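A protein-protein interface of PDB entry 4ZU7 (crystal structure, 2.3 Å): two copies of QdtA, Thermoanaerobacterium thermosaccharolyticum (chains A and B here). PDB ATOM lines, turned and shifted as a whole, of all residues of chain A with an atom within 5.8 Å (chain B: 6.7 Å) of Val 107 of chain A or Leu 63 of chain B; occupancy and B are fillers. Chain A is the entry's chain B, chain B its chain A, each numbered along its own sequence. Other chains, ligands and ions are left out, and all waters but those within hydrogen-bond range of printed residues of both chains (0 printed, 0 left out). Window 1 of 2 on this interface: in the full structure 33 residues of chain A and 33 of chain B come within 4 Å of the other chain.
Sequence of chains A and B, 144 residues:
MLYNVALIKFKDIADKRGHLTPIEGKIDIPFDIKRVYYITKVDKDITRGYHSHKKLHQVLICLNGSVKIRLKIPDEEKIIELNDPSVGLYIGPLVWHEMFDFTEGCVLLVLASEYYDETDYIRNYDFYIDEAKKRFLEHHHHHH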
ATOM      1  N   TYR A  38      10.470  -9.925   3.670  1.00  0.00           N
ATOM      2  CA  TYR A  38      11.223 -10.017   4.897  1.00  0.00           C
ATOM      3  C   TYR A  38      12.162  -8.870   4.987  1.00  0.00           C
ATOM      4  O   TYR A  38      12.691  -8.398   3.981  1.00  0.00           O
ATOM      5  CB  TYR A  38      11.923 -11.388   5.032  1.00  0.00           C
ATOM      6  CG  TYR A  38      12.556 -11.920   3.771  1.00  0.00           C
ATOM      7  CD1 TYR A  38      13.854 -11.558   3.404  1.00  0.00           C
ATOM      8  CD2 TYR A  38      11.875 -12.824   2.953  1.00  0.00           C
ATOM      9  CE1 TYR A  38      14.425 -12.035   2.201  1.00  0.00           C
ATOM     10  CE2 TYR A  38      12.447 -13.335   1.798  1.00  0.00           C
ATOM     11  CZ  TYR A  38      13.710 -12.926   1.398  1.00  0.00           C
ATOM     12  OH  TYR A  38      14.283 -13.458   0.243  1.00  0.00           O
ATOM     13  N   ILE A  39      12.301  -8.393   6.218  1.00  0.00           N
ATOM     14  CA  ILE A  39      13.123  -7.254   6.530  1.00  0.00           C
ATOM     15  C   ILE A  39      14.271  -7.697   7.420  1.00  0.00           C
ATOM     16  O   ILE A  39      14.052  -8.445   8.382  1.00  0.00           O
ATOM     17  CB  ILE A  39      12.303  -6.207   7.271  1.00  0.00           C
ATOM     18  CG1 ILE A  39      11.376  -5.508   6.288  1.00  0.00           C
ATOM     19  CG2 ILE A  39      13.210  -5.208   7.986  1.00  0.00           C
ATOM     20  CD1 ILE A  39      10.182  -4.856   6.970  1.00  0.00           C
ATOM     21  N   THR A  40      15.466  -7.190   7.093  1.00  0.00           N
ATOM     22  CA  THR A  40      16.711  -7.535   7.770  1.00  0.00           C
ATOM     23  C   THR A  40      17.643  -6.347   7.875  1.00  0.00           C
ATOM     24  O   THR A  40      17.556  -5.384   7.090  1.00  0.00           O
ATOM     25  CB  THR A  40      17.545  -8.617   7.035  1.00  0.00           C
ATOM     26  OG1 THR A  40      17.812  -8.221   5.699  1.00  0.00           O
ATOM     27  CG2 THR A  40      16.874  -9.975   7.057  1.00  0.00           C
ATOM     28  N   ILE A  61       6.066 -12.193  11.675  1.00  0.00           N
ATOM     29  CA  ILE A  61       6.780 -13.291  12.335  1.00  0.00           C
ATOM     30  C   ILE A  61       8.241 -12.978  12.423  1.00  0.00           C
ATOM     31  O   ILE A  61       8.886 -12.783  11.380  1.00  0.00           O
ATOM     32  CB  ILE A  61       6.664 -14.645  11.556  1.00  0.00           C
ATOM     33  CG1 ILE A  61       5.208 -15.016  11.191  1.00  0.00           C
ATOM     34  CG2 ILE A  61       7.283 -15.748  12.386  1.00  0.00           C
ATOM     35  CD1 ILE A  61       5.068 -16.182  10.218  1.00  0.00           C
ATOM     36  N   CYS A  62       8.768 -12.925  13.660  1.00  0.00           N
ATOM     37  CA  CYS A  62      10.215 -12.747  13.927  1.00  0.00           C
ATOM     38  C   CYS A  62      10.889 -14.107  13.974  1.00  0.00           C
ATOM     39  O   CYS A  62      10.631 -14.941  14.851  1.00  0.00           O
ATOM     40  CB  CYS A  62      10.491 -12.001  15.258  1.00  0.00           C
ATOM     41  SG  CYS A  62      12.259 -11.609  15.535  1.00  0.00           S
ATOM     42  N   LEU A  63      11.790 -14.334  13.040  1.00  0.00           N
ATOM     43  CA  LEU A  63      12.437 -15.648  12.927  1.00  0.00           C
ATOM     44  C   LEU A  63      13.807 -15.695  13.604  1.00  0.00           C
ATOM     45  O   LEU A  63      14.358 -16.753  13.760  1.00  0.00           O
ATOM     46  CB  LEU A  63      12.598 -16.091  11.463  1.00  0.00           C
ATOM     47  CG  LEU A  63      11.482 -15.901  10.439  1.00  0.00           C
ATOM     48  CD1 LEU A  63      11.946 -16.466   9.100  1.00  0.00           C
ATOM     49  CD2 LEU A  63      10.256 -16.641  10.877  1.00  0.00           C
ATOM     50  N   ASN A  64      14.360 -14.550  13.971  1.00  0.00           N
ATOM     51  CA  ASN A  64      15.617 -14.498  14.713  1.00  0.00           C
ATOM     52  C   ASN A  64      15.606 -13.212  15.456  1.00  0.00           C
ATOM     53  O   ASN A  64      15.001 -12.224  14.998  1.00  0.00           O
ATOM     54  CB  ASN A  64      16.814 -14.543  13.786  1.00  0.00           C
ATOM     55  CG  ASN A  64      18.157 -14.611  14.523  1.00  0.00           C
ATOM     56  OD1 ASN A  64      18.355 -15.420  15.432  1.00  0.00           O
ATOM     57  ND2 ASN A  64      19.111 -13.816  14.062  1.00  0.00           N
ATOM     58  N   GLY A  65      16.254 -13.223  16.612  1.00  0.00           N
ATOM     59  CA  GLY A  65      16.276 -12.068  17.473  1.00  0.00           C
ATOM     60  C   GLY A  65      14.922 -11.587  17.973  1.00  0.00           C
ATOM     61  O   GLY A  65      14.009 -12.360  18.213  1.00  0.00           O
ATOM     62  N   VAL A  67      12.021  -8.070  17.926  1.00  0.00           N
ATOM     63  CA  VAL A  67      11.571  -6.791  17.362  1.00  0.00           C
ATOM     64  C   VAL A  67      10.222  -6.453  17.943  1.00  0.00           C
ATOM     65  O   VAL A  67       9.394  -7.346  18.128  1.00  0.00           O
ATOM     66  CB  VAL A  67      11.521  -6.788  15.799  1.00  0.00           C
ATOM     67  CG1 VAL A  67      10.658  -7.911  15.250  1.00  0.00           C
ATOM     68  CG2 VAL A  67      11.024  -5.452  15.258  1.00  0.00           C
ATOM     69  N   GLY A 105      20.842  -8.871  14.091  1.00  0.00           N
ATOM     70  CA  GLY A 105      20.485 -10.083  13.393  1.00  0.00           C
ATOM     71  C   GLY A 105      18.980 -10.365  13.313  1.00  0.00           C
ATOM     72  O   GLY A 105      18.586 -11.426  12.865  1.00  0.00           O
ATOM     73  N   CYS A 106      18.127  -9.427  13.723  1.00  0.00           N
ATOM     74  CA  CYS A 106      16.681  -9.623  13.560  1.00  0.00           C
ATOM     75  C   CYS A 106      16.290  -9.941  12.102  1.00  0.00           C
ATOM     76  O   CYS A 106      16.802  -9.304  11.176  1.00  0.00           O
ATOM     77  CB  CYS A 106      15.915  -8.403  14.005  1.00  0.00           C
ATOM     78  SG  CYS A 106      14.159  -8.666  14.209  1.00  0.00           S
ATOM     79  N   VAL A 107      15.406 -10.939  11.939  1.00  0.00           N
ATOM     80  CA  VAL A 107      14.694 -11.193  10.712  1.00  0.00           C
ATOM     81  C   VAL A 107      13.185 -11.164  10.997  1.00  0.00           C
ATOM     82  O   VAL A 107      12.673 -11.977  11.796  1.00  0.00           O
ATOM     83  CB  VAL A 107      15.030 -12.564  10.128  1.00  0.00           C
ATOM     84  CG1 VAL A 107      14.365 -12.738   8.777  1.00  0.00           C
ATOM     85  CG2 VAL A 107      16.520 -12.772  10.036  1.00  0.00           C
ATOM     86  N   LEU A 108      12.501 -10.224  10.321  1.00  0.00           N
ATOM     87  CA  LEU A 108      11.052 -10.109  10.267  1.00  0.00           C
ATOM     88  C   LEU A 108      10.453 -10.568   8.898  1.00  0.00           C
ATOM     89  O   LEU A 108      10.732  -9.973   7.827  1.00  0.00           O
ATOM     90  CB  LEU A 108      10.613  -8.670  10.543  1.00  0.00           C
ATOM     91  CG  LEU A 108       9.125  -8.481  10.784  1.00  0.00           C
ATOM     92  CD1 LEU A 108       8.595  -9.155  12.049  1.00  0.00           C
ATOM     93  CD2 LEU A 108       8.821  -7.029  10.861  1.00  0.00           C
ATOM     94  N   LEU A 109       9.620 -11.605   8.981  1.00  0.00           N
ATOM     95  CA  LEU A 109       8.991 -12.240   7.846  1.00  0.00           C
ATOM     96  C   LEU A 109       7.567 -11.796   7.913  1.00  0.00           C
ATOM     97  O   LEU A 109       7.027 -11.718   9.006  1.00  0.00           O
ATOM     98  CB  LEU A 109       9.064 -13.765   7.964  1.00  0.00           C
ATOM     99  CG  LEU A 109       8.293 -14.587   6.922  1.00  0.00           C
ATOM    100  CD1 LEU A 109       8.735 -14.313   5.487  1.00  0.00           C
ATOM    101  CD2 LEU A 109       8.506 -16.060   7.227  1.00  0.00           C
ATOM    102  N   ILE B  23       8.710 -11.255  -2.176  1.00  0.00           N
ATOM    103  CA  ILE B  23       8.507 -12.346  -3.122  1.00  0.00           C
ATOM    104  C   ILE B  23       7.027 -12.578  -3.416  1.00  0.00           C
ATOM    105  O   ILE B  23       6.278 -13.004  -2.533  1.00  0.00           O
ATOM    106  CB  ILE B  23       9.206 -13.600  -2.649  1.00  0.00           C
ATOM    107  CG1 ILE B  23      10.709 -13.304  -2.497  1.00  0.00           C
ATOM    108  CG2 ILE B  23       9.049 -14.724  -3.675  1.00  0.00           C
ATOM    109  CD1 ILE B  23      11.446 -14.219  -1.556  1.00  0.00           C
ATOM    110  N   ILE B  61      15.879 -20.157   0.818  1.00  0.00           N
ATOM    111  CA  ILE B  61      16.469 -18.820   0.995  1.00  0.00           C
ATOM    112  C   ILE B  61      17.039 -18.672   2.400  1.00  0.00           C
ATOM    113  O   ILE B  61      16.333 -18.914   3.436  1.00  0.00           O
ATOM    114  CB  ILE B  61      15.421 -17.705   0.823  1.00  0.00           C
ATOM    115  CG1 ILE B  61      14.554 -17.949  -0.406  1.00  0.00           C
ATOM    116  CG2 ILE B  61      16.074 -16.339   0.700  1.00  0.00           C
ATOM    117  CD1 ILE B  61      13.376 -17.028  -0.505  1.00  0.00           C
ATOM    118  N   CYS B  62      18.304 -18.271   2.470  1.00  0.00           N
ATOM    119  CA  CYS B  62      18.926 -18.061   3.785  1.00  0.00           C
ATOM    120  C   CYS B  62      18.843 -16.593   4.061  1.00  0.00           C
ATOM    121  O   CYS B  62      19.515 -15.822   3.391  1.00  0.00           O
ATOM    122  CB  CYS B  62      20.387 -18.507   3.841  1.00  0.00           C
ATOM    123  SG  CYS B  62      21.170 -18.164   5.454  1.00  0.00           S
ATOM    124  N   LEU B  63      18.051 -16.227   5.071  1.00  0.00           N
ATOM    125  CA  LEU B  63      17.830 -14.844   5.474  1.00  0.00           C
ATOM    126  C   LEU B  63      18.735 -14.299   6.601  1.00  0.00           C
ATOM    127  O   LEU B  63      18.611 -13.146   6.928  1.00  0.00           O
ATOM    128  CB  LEU B  63      16.392 -14.693   5.989  1.00  0.00           C
ATOM    129  CG  LEU B  63      15.242 -15.401   5.271  1.00  0.00           C
ATOM    130  CD1 LEU B  63      13.929 -14.943   5.860  1.00  0.00           C
ATOM    131  CD2 LEU B  63      15.300 -15.058   3.803  1.00  0.00           C
ATOM    132  N   ASN B  64      19.514 -15.147   7.270  1.00  0.00           N
ATOM    133  CA  ASN B  64      20.510 -14.726   8.261  1.00  0.00           C
ATOM    134  C   ASN B  64      21.679 -15.732   8.350  1.00  0.00           C
ATOM    135  O   ASN B  64      21.474 -16.944   8.295  1.00  0.00           O
ATOM    136  CB  ASN B  64      19.925 -14.541   9.655  1.00  0.00           C
ATOM    137  CG  ASN B  64      20.874 -13.794  10.581  1.00  0.00           C
ATOM    138  OD1 ASN B  64      21.071 -14.170  11.729  1.00  0.00           O
ATOM    139  ND2 ASN B  64      21.439 -12.714  10.087  1.00  0.00           N
ATOM    140  N   GLY B  65      22.902 -15.209   8.457  1.00  0.00           N
ATOM    141  CA  GLY B  65      24.070 -16.046   8.514  1.00  0.00           C
ATOM    142  C   GLY B  65      24.170 -16.817   7.216  1.00  0.00           C
ATOM    143  O   GLY B  65      23.887 -16.271   6.144  1.00  0.00           O
ATOM    144  N   ASP B  84      23.027 -14.723   1.242  1.00  0.00           N
ATOM    145  CA  ASP B  84      22.448 -13.496   0.760  1.00  0.00           C
ATOM    146  C   ASP B  84      20.933 -13.709   0.676  1.00  0.00           C
ATOM    147  O   ASP B  84      20.496 -14.504  -0.154  1.00  0.00           O
ATOM    148  CB  ASP B  84      22.984 -13.184  -0.616  1.00  0.00           C
ATOM    149  CG  ASP B  84      22.550 -11.826  -1.137  1.00  0.00           C
ATOM    150  OD1 ASP B  84      21.419 -11.331  -0.829  1.00  0.00           O
ATOM    151  OD2 ASP B  84      23.372 -11.282  -1.909  1.00  0.00           O
ATOM    152  N   PRO B  85      20.155 -12.996   1.545  1.00  0.00           N
ATOM    153  CA  PRO B  85      18.731 -13.068   1.630  1.00  0.00           C
ATOM    154  C   PRO B  85      18.025 -12.743   0.343  1.00  0.00           C
ATOM    155  O   PRO B  85      16.870 -13.162   0.136  1.00  0.00           O
ATOM    156  CB  PRO B  85      18.387 -12.009   2.721  1.00  0.00           C
ATOM    157  CG  PRO B  85      19.580 -11.988   3.636  1.00  0.00           C
ATOM    158  CD  PRO B  85      20.714 -12.125   2.622  1.00  0.00           C
ATOM    159  N   SER B  86      18.704 -12.072  -0.557  1.00  0.00           N
ATOM    160  CA  SER B  86      18.073 -11.699  -1.792  1.00  0.00           C
ATOM    161  C   SER B  86      18.350 -12.675  -2.957  1.00  0.00           C
ATOM    162  O   SER B  86      18.053 -12.353  -4.118  1.00  0.00           O
ATOM    163  CB  SER B  86      18.534 -10.309  -2.178  1.00  0.00           C
ATOM    164  OG  SER B  86      19.653 -10.450  -3.024  1.00  0.00           O
ATOM    165  N   GLY B 105      22.895 -18.255  14.540  1.00  0.00           N
ATOM    166  CA  GLY B 105      21.789 -17.397  14.069  1.00  0.00           C
ATOM    167  C   GLY B 105      21.164 -17.662  12.687  1.00  0.00           C
ATOM    168  O   GLY B 105      20.268 -16.941  12.278  1.00  0.00           O
ATOM    169  N   CYS B 106      21.624 -18.680  11.962  1.00  0.00           N
ATOM    170  CA  CYS B 106      21.125 -18.949  10.614  1.00  0.00           C
ATOM    171  C   CYS B 106      19.631 -19.153  10.605  1.00  0.00           C
ATOM    172  O   CYS B 106      19.103 -19.750  11.542  1.00  0.00           O
ATOM    173  CB  CYS B 106      21.769 -20.198  10.061  1.00  0.00           C
ATOM    174  SG  CYS B 106      21.267 -20.640   8.389  1.00  0.00           S
ATOM    175  N   VAL B 107      18.985 -18.678   9.524  1.00  0.00           N
ATOM    176  CA  VAL B 107      17.573 -18.850   9.241  1.00  0.00           C
ATOM    177  C   VAL B 107      17.413 -19.274   7.791  1.00  0.00           C
ATOM    178  O   VAL B 107      17.803 -18.559   6.895  1.00  0.00           O
ATOM    179  CB  VAL B 107      16.772 -17.541   9.408  1.00  0.00           C
ATOM    180  CG1 VAL B 107      15.280 -17.796   9.124  1.00  0.00           C
ATOM    181  CG2 VAL B 107      16.976 -16.900  10.781  1.00  0.00           C
ATOM    182  N   LEU B 108      16.872 -20.469   7.589  1.00  0.00           N
ATOM    183  CA  LEU B 108      16.578 -21.022   6.291  1.00  0.00           C
ATOM    184  C   LEU B 108      15.044 -21.030   6.130  1.00  0.00           C
ATOM    185  O   LEU B 108      14.284 -21.539   6.996  1.00  0.00           O
ATOM    186  CB  LEU B 108      17.114 -22.453   6.207  1.00  0.00           C
ATOM    187  CG  LEU B 108      17.051 -23.104   4.825  1.00  0.00           C
ATOM    188  CD1 LEU B 108      17.705 -22.261   3.725  1.00  0.00           C
ATOM    189  CD2 LEU B 108      17.687 -24.500   4.879  1.00  0.00           C
ATOM    190  N   LEU B 109      14.608 -20.417   5.047  1.00  0.00           N
ATOM    191  CA  LEU B 109      13.214 -20.286   4.720  1.00  0.00           C
ATOM    192  C   LEU B 109      13.059 -21.009   3.422  1.00  0.00           C
ATOM    193  O   LEU B 109      13.907 -20.905   2.526  1.00  0.00           O
ATOM    194  CB  LEU B 109      12.881 -18.837   4.492  1.00  0.00           C
ATOM    195  CG  LEU B 109      11.546 -18.543   3.858  1.00  0.00           C
ATOM    196  CD1 LEU B 109      10.438 -18.979   4.809  1.00  0.00           C
ATOM    197  CD2 LEU B 109      11.482 -17.057   3.582  1.00  0.00           C
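Leu 63 of chain A touches Val 107 of chain B, and with the chains exchanged Val 107 of chain A touches Leu 63 of chain B.
Asn 64 of chain B touches its own counterpart, Asn 64 of chain A.
Asn 64 of chain A touches Gly 105 of chain B, and with the chains exchanged Gly 105 of chain A touches Asn 64 of chain B.
Asn 64 of chain A touches Val 107 of chain B, and with the chains exchanged Val 107 of chain A touches Asn 64 of chain B.
Of the 12 pairs that touch across the chains among the printed residues, 7 have their exchanged pair printed and touching as well.
The side-chain amide nitrogen of Asn 64 of chain A sits at hydrogen-bond distance from the side-chain amide oxygen of Asn 64 of chain B, at 3.1 Å.
The backbone carbonyl oxygen (O) of Pro 85 of chain B is in hydrogen-bond range of the side-chain hydroxyl (OH) of Tyr 38 of chain A.
The backbone carbonyl oxygen (O) of Asn 64 of chain B lies within hydrogen-bond range of the side-chain sulfur (SG) of Cys 62 of chain B, at 3.1 Å.
N of Val 107 of chain B sits at hydrogen-bond distance from O of Asn 64 of chain B, 3.3 Å away.
SG of Cys 62 of chain A is in hydrogen-bond range of O of Asn 64 of chain A.
O of Val 107 of chain A lies within hydrogen-bond range of N of Leu 63 of chain A (2.8 Å).
The side-chain amide nitrogen (ND2) of Asn 64 of chain A is in hydrogen-bond range of the backbone carbonyl oxygen (O) of Gly 105 of chain A.
The backbone NH (N) of Val 107 of chain A lies within hydrogen-bond range of the backbone carbonyl oxygen (O) of Asn 64 of chain A (3.3 Å).
Of the 14 printed residues of chain A, 6 touch a printed residue of chain B.
Printed residues of chain B that touch a printed residue of chain A: Ile 23, Ile 61, Leu 63, Asn 64, Pro 85, Gly 105 and Val 107.
Hydrophobic or aromatic side chains of chain B within 4 Å of the printed part of chain A: Ile 23, Ile 61, Leu 63, Pro 85 and Val 107.
Among the printed residues, merely in contact across the chains: Tyr 38 of chain A with Ile 61 of chain B (3.4 Å), Tyr 38 of chain A with Ile 23 of chain B (3.4 Å), Tyr 38 of chain A with Leu 63 of chain B (3.5 Å), Leu 63 of chain A with Val 107 of chain B (3.6 Å), Thr 40 of chain A with Leu 63 of chain B (3.6 Å), Val 107 of chain A with Leu 63 of chain B (3.7 Å), Asn 64 of chain A with Gly 105 of chain B (3.8 Å), Asn 64 of chain A with Val 107 of chain B (3.8 Å), Val 107 of chain A with Asn 64 of chain B (3.9 Å) and Gly 105 of chain A with Asn 64 of chain B (3.9 Å).
Leu 63 of chain B touches just these residues of chain A: Tyr 38, Thr 40 and Val 107.
Of the printed residues of chain A, Gly 105 of chain B touches Asn 64.
Printed residues of chain A within 4 Å of Val 107 of chain B: Leu 63 (3.6 Å) and Asn 64 (3.8 Å).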
